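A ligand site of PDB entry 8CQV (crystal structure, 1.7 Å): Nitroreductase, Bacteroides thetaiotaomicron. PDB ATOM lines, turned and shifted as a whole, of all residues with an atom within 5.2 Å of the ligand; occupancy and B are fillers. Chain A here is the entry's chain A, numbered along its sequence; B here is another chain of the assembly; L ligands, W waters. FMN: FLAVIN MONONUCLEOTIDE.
OG1 of Thr 16 lies within hydrogen-bond range of O3P of the ligand (2.7 Å). The backbone NH of Thr 16 lies within hydrogen-bond range of an oxygen (O1P) of the ligand, 2.8 Å away. A ring nitrogen (ND1) of His 152 lies within hydrogen-bond range of an oxygen (O4) of the ligand, 3.0 Å away. NE2 of Gln 151 sits at hydrogen-bond distance from O2 of the ligand, at 3.0 Å. NZ of Lys 189 is in salt-bridge range of O2P of the ligand, at 2.7 Å. The side-chain hydroxyl (OH) of Tyr 18 lies within hydrogen-bond range of an oxygen (O2) of the ligand (2.5 Å). O1P of the ligand is in salt-bridge range of NE of Arg 15 (2.9 Å). The guanidinium group (NH2) of Arg 14 is in salt-bridge range of an oxygen (O2P) of the ligand (2.7 Å). A nitrogen (N3) of the ligand sits close to the backbone carbonyl oxygen (O) of Leu 150 (3.1 Å).
Water W4 lies within hydrogen-bond range of an oxygen (O1P) of the ligand and the guanidinium group of Arg 15. Water W1 bridges an oxygen (O2') of the ligand (2.7 Å) and the backbone NH of Phe 46 of chain B (2.8 Å). Water W2 lies within hydrogen-bond range of OG1 of Thr 16 (2.9 Å), N of Leu 150 (2.9 Å) and N1 of the ligand (2.9 Å). Water W3 lies within hydrogen-bond range of OE1 of Gln 151, N of His 152 and O4 of the ligand.
The guanidinium group (NH2) of Arg 14 sits at hydrogen-bond distance from the backbone carbonyl oxygen (O) of His 41 of chain B (3.1 Å). The side-chain hydroxyl of Ser 149 is in hydrogen-bond range of the side-chain amide nitrogen of Gln 151 (2.9 Å). The backbone carbonyl oxygen (O) of Pro 43 of chain B is in hydrogen-bond range of the side-chain hydroxyl (OG1) of Thr 129 of chain B, 2.7 Å away.
CH2 of Trp 138 touches O3' of the ligand, 3.9 Å away. CB of Pro 43 of chain B touches O3' of the ligand (3.1 Å). Ser 44 of chain B touches the ligand (O to C2', 3.4 Å). Ala 45 of chain B touches the ligand. Phe 46 of chain B touches the ligand. Asn 47 of chain B touches the ligand. Trp 125 of chain B touches the ligand (CD1 to C7M, 3.8 Å). The nearest printed residue that does not touch the ligand is Met 132 of chain B (4.3 Å).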
ATOM      1  N   ARG A  14     -13.891  10.595 -28.702  1.00  0.00           N
ATOM      2  CA  ARG A  14     -13.376   9.260 -28.471  1.00  0.00           C
ATOM      3  C   ARG A  14     -14.531   8.235 -28.473  1.00  0.00           C
ATOM      4  O   ARG A  14     -15.482   8.353 -27.730  1.00  0.00           O
ATOM      5  CB  ARG A  14     -12.546   9.228 -27.196  1.00  0.00           C
ATOM      6  CG  ARG A  14     -12.027   7.813 -26.836  1.00  0.00           C
ATOM      7  CD  ARG A  14     -12.246   7.481 -25.388  1.00  0.00           C
ATOM      8  NE  ARG A  14     -13.631   7.454 -24.990  1.00  0.00           N
ATOM      9  CZ  ARG A  14     -14.553   6.561 -25.369  1.00  0.00           C
ATOM     10  NH1 ARG A  14     -14.275   5.391 -25.984  1.00  0.00           N
ATOM     11  NH2 ARG A  14     -15.790   6.801 -25.007  1.00  0.00           N
ATOM     12  N   ARG A  15     -14.441   7.213 -29.314  1.00  0.00           N
ATOM     13  CA  ARG A  15     -15.413   6.137 -29.363  1.00  0.00           C
ATOM     14  C   ARG A  15     -14.658   4.821 -29.574  1.00  0.00           C
ATOM     15  O   ARG A  15     -13.495   4.812 -29.981  1.00  0.00           O
ATOM     16  CB  ARG A  15     -16.400   6.377 -30.529  1.00  0.00           C
ATOM     17  CG  ARG A  15     -17.356   7.566 -30.327  1.00  0.00           C
ATOM     18  CD  ARG A  15     -18.308   7.365 -29.187  1.00  0.00           C
ATOM     19  NE  ARG A  15     -19.163   6.227 -29.343  1.00  0.00           N
ATOM     20  CZ  ARG A  15     -20.163   6.123 -30.199  1.00  0.00           C
ATOM     21  NH1 ARG A  15     -20.624   7.198 -30.860  1.00  0.00           N
ATOM     22  NH2 ARG A  15     -20.814   4.987 -30.310  1.00  0.00           N
ATOM     23  N   THR A  16     -15.375   3.688 -29.379  1.00  0.00           N
ATOM     24  CA  THR A  16     -14.832   2.385 -29.699  1.00  0.00           C
ATOM     25  C   THR A  16     -14.942   2.165 -31.209  1.00  0.00           C
ATOM     26  O   THR A  16     -16.042   2.284 -31.759  1.00  0.00           O
ATOM     27  CB  THR A  16     -15.561   1.275 -28.927  1.00  0.00           C
ATOM     28  OG1 THR A  16     -15.238   1.404 -27.544  1.00  0.00           O
ATOM     29  CG2 THR A  16     -15.209  -0.116 -29.402  1.00  0.00           C
ATOM     30  N   TYR A  18     -13.951  -0.914 -34.038  1.00  0.00           N
ATOM     31  CA  TYR A  18     -13.506  -2.254 -34.377  1.00  0.00           C
ATOM     32  C   TYR A  18     -13.029  -2.312 -35.820  1.00  0.00           C
ATOM     33  O   TYR A  18     -12.208  -3.186 -36.121  1.00  0.00           O
ATOM     34  CB  TYR A  18     -14.654  -3.244 -34.133  1.00  0.00           C
ATOM     35  CG  TYR A  18     -15.099  -3.307 -32.691  1.00  0.00           C
ATOM     36  CD1 TYR A  18     -14.204  -3.548 -31.662  1.00  0.00           C
ATOM     37  CD2 TYR A  18     -16.411  -3.093 -32.312  1.00  0.00           C
ATOM     38  CE1 TYR A  18     -14.582  -3.600 -30.343  1.00  0.00           C
ATOM     39  CE2 TYR A  18     -16.812  -3.083 -30.983  1.00  0.00           C
ATOM     40  CZ  TYR A  18     -15.898  -3.384 -29.993  1.00  0.00           C
ATOM     41  OH  TYR A  18     -16.275  -3.450 -28.676  1.00  0.00           O
ATOM     42  N   TRP A 138      -6.110   6.675 -25.379  1.00  0.00           N
ATOM     43  CA  TRP A 138      -7.277   6.421 -26.218  1.00  0.00           C
ATOM     44  C   TRP A 138      -7.730   7.701 -26.923  1.00  0.00           C
ATOM     45  O   TRP A 138      -7.916   7.728 -28.141  1.00  0.00           O
ATOM     46  CB  TRP A 138      -8.403   5.779 -25.428  1.00  0.00           C
ATOM     47  CG  TRP A 138      -9.404   5.024 -26.207  1.00  0.00           C
ATOM     48  CD1 TRP A 138      -9.611   4.974 -27.563  1.00  0.00           C
ATOM     49  CD2 TRP A 138     -10.423   4.211 -25.620  1.00  0.00           C
ATOM     50  NE1 TRP A 138     -10.701   4.168 -27.829  1.00  0.00           N
ATOM     51  CE2 TRP A 138     -11.197   3.695 -26.655  1.00  0.00           C
ATOM     52  CE3 TRP A 138     -10.767   3.911 -24.304  1.00  0.00           C
ATOM     53  CZ2 TRP A 138     -12.276   2.849 -26.406  1.00  0.00           C
ATOM     54  CZ3 TRP A 138     -11.814   3.081 -24.060  1.00  0.00           C
ATOM     55  CH2 TRP A 138     -12.589   2.607 -25.090  1.00  0.00           C
ATOM     56  N   SER A 149      -9.851   0.436 -29.832  1.00  0.00           N
ATOM     57  CA  SER A 149     -10.735  -0.193 -28.842  1.00  0.00           C
ATOM     58  C   SER A 149      -9.889  -0.566 -27.629  1.00  0.00           C
ATOM     59  O   SER A 149      -8.660  -0.485 -27.638  1.00  0.00           O
ATOM     60  CB  SER A 149     -11.460  -1.362 -29.411  1.00  0.00           C
ATOM     61  OG  SER A 149     -10.535  -2.377 -29.758  1.00  0.00           O
ATOM     62  N   LEU A 150     -10.578  -0.948 -26.558  1.00  0.00           N
ATOM     63  CA  LEU A 150      -9.944  -1.326 -25.311  1.00  0.00           C
ATOM     64  C   LEU A 150     -10.280  -2.771 -25.015  1.00  0.00           C
ATOM     65  O   LEU A 150     -11.451  -3.104 -24.793  1.00  0.00           O
ATOM     66  CB  LEU A 150     -10.439  -0.430 -24.201  1.00  0.00           C
ATOM     67  CG  LEU A 150      -9.759  -0.641 -22.843  1.00  0.00           C
ATOM     68  CD1 LEU A 150      -8.310  -0.183 -22.894  1.00  0.00           C
ATOM     69  CD2 LEU A 150     -10.483   0.157 -21.759  1.00  0.00           C
ATOM     70  N   GLN A 151      -9.275  -3.651 -25.036  1.00  0.00           N
ATOM     71  CA  GLN A 151      -9.509  -5.077 -24.927  1.00  0.00           C
ATOM     72  C   GLN A 151      -8.900  -5.630 -23.650  1.00  0.00           C
ATOM     73  O   GLN A 151      -7.967  -5.067 -23.070  1.00  0.00           O
ATOM     74  CB  GLN A 151      -8.928  -5.812 -26.158  1.00  0.00           C
ATOM     75  CG  GLN A 151      -9.556  -5.359 -27.438  1.00  0.00           C
ATOM     76  CD  GLN A 151     -11.056  -5.441 -27.451  1.00  0.00           C
ATOM     77  OE1 GLN A 151     -11.637  -6.398 -26.897  1.00  0.00           O
ATOM     78  NE2 GLN A 151     -11.677  -4.431 -28.030  1.00  0.00           N
ATOM     79  N   HIS A 152      -9.466  -6.737 -23.207  1.00  0.00           N
ATOM     80  CA  HIS A 152      -9.035  -7.445 -22.002  1.00  0.00           C
ATOM     81  C   HIS A 152      -8.913  -8.949 -22.257  1.00  0.00           C
ATOM     82  O   HIS A 152      -9.696  -9.790 -21.725  1.00  0.00           O
ATOM     83  CB  HIS A 152     -10.046  -7.152 -20.892  1.00  0.00           C
ATOM     84  CG  HIS A 152     -10.122  -5.698 -20.561  1.00  0.00           C
ATOM     85  ND1 HIS A 152     -10.933  -4.818 -21.249  1.00  0.00           N
ATOM     86  CD2 HIS A 152      -9.363  -4.971 -19.750  1.00  0.00           C
ATOM     87  CE1 HIS A 152     -10.707  -3.595 -20.744  1.00  0.00           C
ATOM     88  NE2 HIS A 152      -9.775  -3.641 -19.849  1.00  0.00           N
ATOM     89  N   LYS A 189     -24.992   4.572 -29.427  1.00  0.00           N
ATOM     90  CA  LYS A 189     -24.631   4.486 -28.019  1.00  0.00           C
ATOM     91  C   LYS A 189     -25.823   4.966 -27.215  1.00  0.00           C
ATOM     92  O   LYS A 189     -26.283   6.092 -27.410  1.00  0.00           O
ATOM     93  CB  LYS A 189     -23.403   5.342 -27.775  1.00  0.00           C
ATOM     94  CG  LYS A 189     -22.838   5.313 -26.367  1.00  0.00           C
ATOM     95  CD  LYS A 189     -21.558   6.117 -26.265  1.00  0.00           C
ATOM     96  CE  LYS A 189     -21.080   6.226 -24.843  1.00  0.00           C
ATOM     97  NZ  LYS A 189     -19.764   6.892 -24.714  1.00  0.00           N
ATOM     98  N   HIS B  41     -19.607  11.129 -21.809  1.00  0.00           N
ATOM     99  CA  HIS B  41     -18.668  10.600 -22.812  1.00  0.00           C
ATOM    100  C   HIS B  41     -17.566   9.671 -22.279  1.00  0.00           C
ATOM    101  O   HIS B  41     -16.885   9.057 -23.130  1.00  0.00           O
ATOM    102  CB  HIS B  41     -18.106  11.742 -23.659  1.00  0.00           C
ATOM    103  CG  HIS B  41     -19.187  12.495 -24.371  1.00  0.00           C
ATOM    104  ND1 HIS B  41     -20.173  11.930 -25.181  1.00  0.00           N
ATOM    105  CD2 HIS B  41     -19.520  13.803 -24.267  1.00  0.00           C
ATOM    106  CE1 HIS B  41     -21.033  12.906 -25.555  1.00  0.00           C
ATOM    107  NE2 HIS B  41     -20.634  14.043 -24.994  1.00  0.00           N
ATOM    108  N   PRO B  43     -15.911   6.464 -21.081  1.00  0.00           N
ATOM    109  CA  PRO B  43     -16.455   5.122 -21.342  1.00  0.00           C
ATOM    110  C   PRO B  43     -16.570   4.286 -20.067  1.00  0.00           C
ATOM    111  O   PRO B  43     -15.796   4.490 -19.160  1.00  0.00           O
ATOM    112  CB  PRO B  43     -15.446   4.501 -22.334  1.00  0.00           C
ATOM    113  CG  PRO B  43     -14.144   5.199 -22.000  1.00  0.00           C
ATOM    114  CD  PRO B  43     -14.557   6.663 -21.675  1.00  0.00           C
ATOM    115  N   SER B  44     -17.410   3.247 -20.156  1.00  0.00           N
ATOM    116  CA  SER B  44     -17.580   2.213 -19.137  1.00  0.00           C
ATOM    117  C   SER B  44     -17.705   0.865 -19.819  1.00  0.00           C
ATOM    118  O   SER B  44     -18.249   0.754 -20.891  1.00  0.00           O
ATOM    119  CB  SER B  44     -18.745   2.465 -18.211  1.00  0.00           C
ATOM    120  OG  SER B  44     -19.931   2.758 -18.983  1.00  0.00           O
ATOM    121  N   ALA B  45     -17.302  -0.179 -19.079  1.00  0.00           N
ATOM    122  CA  ALA B  45     -17.468  -1.543 -19.575  1.00  0.00           C
ATOM    123  C   ALA B  45     -18.936  -1.881 -19.869  1.00  0.00           C
ATOM    124  O   ALA B  45     -19.827  -1.510 -19.080  1.00  0.00           O
ATOM    125  CB  ALA B  45     -16.961  -2.533 -18.609  1.00  0.00           C
ATOM    126  N   PHE B  46     -19.179  -2.512 -21.031  1.00  0.00           N
ATOM    127  CA  PHE B  46     -20.519  -2.869 -21.489  1.00  0.00           C
ATOM    128  C   PHE B  46     -21.413  -1.630 -21.624  1.00  0.00           C
ATOM    129  O   PHE B  46     -22.623  -1.769 -21.604  1.00  0.00           O
ATOM    130  CB  PHE B  46     -21.172  -3.904 -20.553  1.00  0.00           C
ATOM    131  CG  PHE B  46     -20.655  -5.318 -20.609  1.00  0.00           C
ATOM    132  CD1 PHE B  46     -19.312  -5.629 -20.462  1.00  0.00           C
ATOM    133  CD2 PHE B  46     -21.536  -6.374 -20.745  1.00  0.00           C
ATOM    134  CE1 PHE B  46     -18.866  -6.951 -20.477  1.00  0.00           C
ATOM    135  CE2 PHE B  46     -21.083  -7.692 -20.788  1.00  0.00           C
ATOM    136  CZ  PHE B  46     -19.742  -7.962 -20.687  1.00  0.00           C
ATOM    137  N   ASN B  47     -20.867  -0.399 -21.742  1.00  0.00           N
ATOM    138  CA  ASN B  47     -21.648   0.800 -21.690  1.00  0.00           C
ATOM    139  C   ASN B  47     -22.551   0.845 -20.450  1.00  0.00           C
ATOM    140  O   ASN B  47     -23.707   1.275 -20.520  1.00  0.00           O
ATOM    141  CB  ASN B  47     -22.474   1.005 -22.986  1.00  0.00           C
ATOM    142  CG  ASN B  47     -22.956   2.454 -23.093  1.00  0.00           C
ATOM    143  OD1 ASN B  47     -22.341   3.370 -22.529  1.00  0.00           O
ATOM    144  ND2 ASN B  47     -24.148   2.635 -23.647  1.00  0.00           N
ATOM    145  N   TRP B 125     -13.458  -2.952 -13.271  1.00  0.00           N
ATOM    146  CA  TRP B 125     -13.841  -2.090 -14.380  1.00  0.00           C
ATOM    147  C   TRP B 125     -14.639  -0.864 -13.913  1.00  0.00           C
ATOM    148  O   TRP B 125     -14.514   0.208 -14.492  1.00  0.00           O
ATOM    149  CB  TRP B 125     -14.613  -2.878 -15.406  1.00  0.00           C
ATOM    150  CG  TRP B 125     -13.800  -3.810 -16.233  1.00  0.00           C
ATOM    151  CD1 TRP B 125     -12.449  -3.725 -16.478  1.00  0.00           C
ATOM    152  CD2 TRP B 125     -14.288  -4.925 -16.999  1.00  0.00           C
ATOM    153  NE1 TRP B 125     -12.083  -4.722 -17.315  1.00  0.00           N
ATOM    154  CE2 TRP B 125     -13.141  -5.491 -17.641  1.00  0.00           C
ATOM    155  CE3 TRP B 125     -15.539  -5.544 -17.152  1.00  0.00           C
ATOM    156  CZ2 TRP B 125     -13.256  -6.564 -18.526  1.00  0.00           C
ATOM    157  CZ3 TRP B 125     -15.633  -6.595 -18.036  1.00  0.00           C
ATOM    158  CH2 TRP B 125     -14.507  -7.077 -18.723  1.00  0.00           C
ATOM    159  N   GLN B 128     -12.120   1.502 -12.570  1.00  0.00           N
ATOM    160  CA  GLN B 128     -11.451   2.083 -13.700  1.00  0.00           C
ATOM    161  C   GLN B 128     -12.218   3.227 -14.367  1.00  0.00           C
ATOM    162  O   GLN B 128     -11.648   4.308 -14.593  1.00  0.00           O
ATOM    163  CB  GLN B 128     -11.048   0.988 -14.658  1.00  0.00           C
ATOM    164  CG  GLN B 128      -9.895   0.132 -14.133  1.00  0.00           C
ATOM    165  CD  GLN B 128      -9.574  -0.884 -15.237  1.00  0.00           C
ATOM    166  OE1 GLN B 128      -9.012  -0.507 -16.242  1.00  0.00           O
ATOM    167  NE2 GLN B 128      -9.803  -2.161 -15.065  1.00  0.00           N
ATOM    168  N   THR B 129     -13.514   3.039 -14.612  1.00  0.00           N
ATOM    169  CA  THR B 129     -14.308   4.084 -15.246  1.00  0.00           C
ATOM    170  C   THR B 129     -14.371   5.245 -14.250  1.00  0.00           C
ATOM    171  O   THR B 129     -14.239   6.379 -14.630  1.00  0.00           O
ATOM    172  CB  THR B 129     -15.716   3.641 -15.716  1.00  0.00           C
ATOM    173  OG1 THR B 129     -16.271   4.708 -16.507  1.00  0.00           O
ATOM    174  CG2 THR B 129     -16.636   3.204 -14.614  1.00  0.00           C
ATOM    175  N   MET B 132     -11.243   7.237 -14.705  1.00  0.00           N
ATOM    176  CA  MET B 132     -11.291   7.946 -15.980  1.00  0.00           C
ATOM    177  C   MET B 132     -12.128   9.264 -15.816  1.00  0.00           C
ATOM    178  O   MET B 132     -11.717  10.292 -16.295  1.00  0.00           O
ATOM    179  CB  MET B 132     -11.823   7.095 -17.123  1.00  0.00           C
ATOM    180  CG  MET B 132     -10.924   5.923 -17.532  1.00  0.00           C
ATOM    181  SD  MET B 132     -11.636   5.028 -18.836  1.00  0.00           S
ATOM    182  CE  MET B 132     -10.440   3.720 -19.147  1.00  0.00           C
HETATM  183  N1  FMN L   1     -14.730  -2.986 -25.389  1.00  0.00           N
HETATM  184  C2  FMN L   1     -14.377  -4.183 -25.876  1.00  0.00           C
HETATM  185  O2  FMN L   1     -14.551  -4.449 -27.092  1.00  0.00           O
HETATM  186  N3  FMN L   1     -13.807  -5.146 -25.111  1.00  0.00           N
HETATM  187  C4  FMN L   1     -13.585  -4.992 -23.782  1.00  0.00           C
HETATM  188  O4  FMN L   1     -12.950  -5.847 -23.180  1.00  0.00           O
HETATM  189  C4A FMN L   1     -13.959  -3.779 -23.197  1.00  0.00           C
HETATM  190  N5  FMN L   1     -13.793  -3.588 -21.897  1.00  0.00           N
HETATM  191  C5A FMN L   1     -13.878  -2.288 -21.420  1.00  0.00           C
HETATM  192  C6  FMN L   1     -13.489  -2.011 -20.112  1.00  0.00           C
HETATM  193  C7  FMN L   1     -13.559  -0.734 -19.613  1.00  0.00           C
HETATM  194  C7M FMN L   1     -13.187  -0.460 -18.178  1.00  0.00           C
HETATM  195  C8  FMN L   1     -14.081   0.270 -20.412  1.00  0.00           C
HETATM  196  C8M FMN L   1     -14.124   1.653 -19.901  1.00  0.00           C
HETATM  197  C9  FMN L   1     -14.428   0.041 -21.683  1.00  0.00           C
HETATM  198  C9A FMN L   1     -14.422  -1.228 -22.217  1.00  0.00           C
HETATM  199  N10 FMN L   1     -14.811  -1.554 -23.524  1.00  0.00           N
HETATM  200  C10 FMN L   1     -14.534  -2.795 -24.083  1.00  0.00           C
HETATM  201  C1' FMN L   1     -15.439  -0.566 -24.399  1.00  0.00           C
HETATM  202  C2' FMN L   1     -16.936  -0.219 -23.883  1.00  0.00           C
HETATM  203  O2' FMN L   1     -17.883  -1.260 -24.046  1.00  0.00           O
HETATM  204  C3' FMN L   1     -17.309   1.087 -24.538  1.00  0.00           C
HETATM  205  O3' FMN L   1     -16.354   2.127 -24.126  1.00  0.00           O
HETATM  206  C4' FMN L   1     -18.752   1.560 -24.227  1.00  0.00           C
HETATM  207  O4' FMN L   1     -19.674   0.680 -24.889  1.00  0.00           O
HETATM  208  C5' FMN L   1     -19.004   2.960 -24.735  1.00  0.00           C
HETATM  209  O5' FMN L   1     -18.759   3.011 -26.149  1.00  0.00           O
HETATM  210  P   FMN L   1     -17.677   4.102 -26.657  1.00  0.00           P
HETATM  211  O1P FMN L   1     -17.859   3.974 -28.127  1.00  0.00           O
HETATM  212  O2P FMN L   1     -17.933   5.455 -26.013  1.00  0.00           O
HETATM  213  O3P FMN L   1     -16.279   3.483 -26.188  1.00  0.00           O
HETATM  214  O   HOH W   1     -17.352  -3.645 -22.846  1.00  0.00           O
HETATM  215  O   HOH W   2     -13.456  -0.732 -26.793  1.00  0.00           O
HETATM  216  O   HOH W   3     -11.653  -8.460 -24.702  1.00  0.00           O
HETATM  217  O   HOH W   4     -19.990   2.696 -29.094  1.00  0.00           O
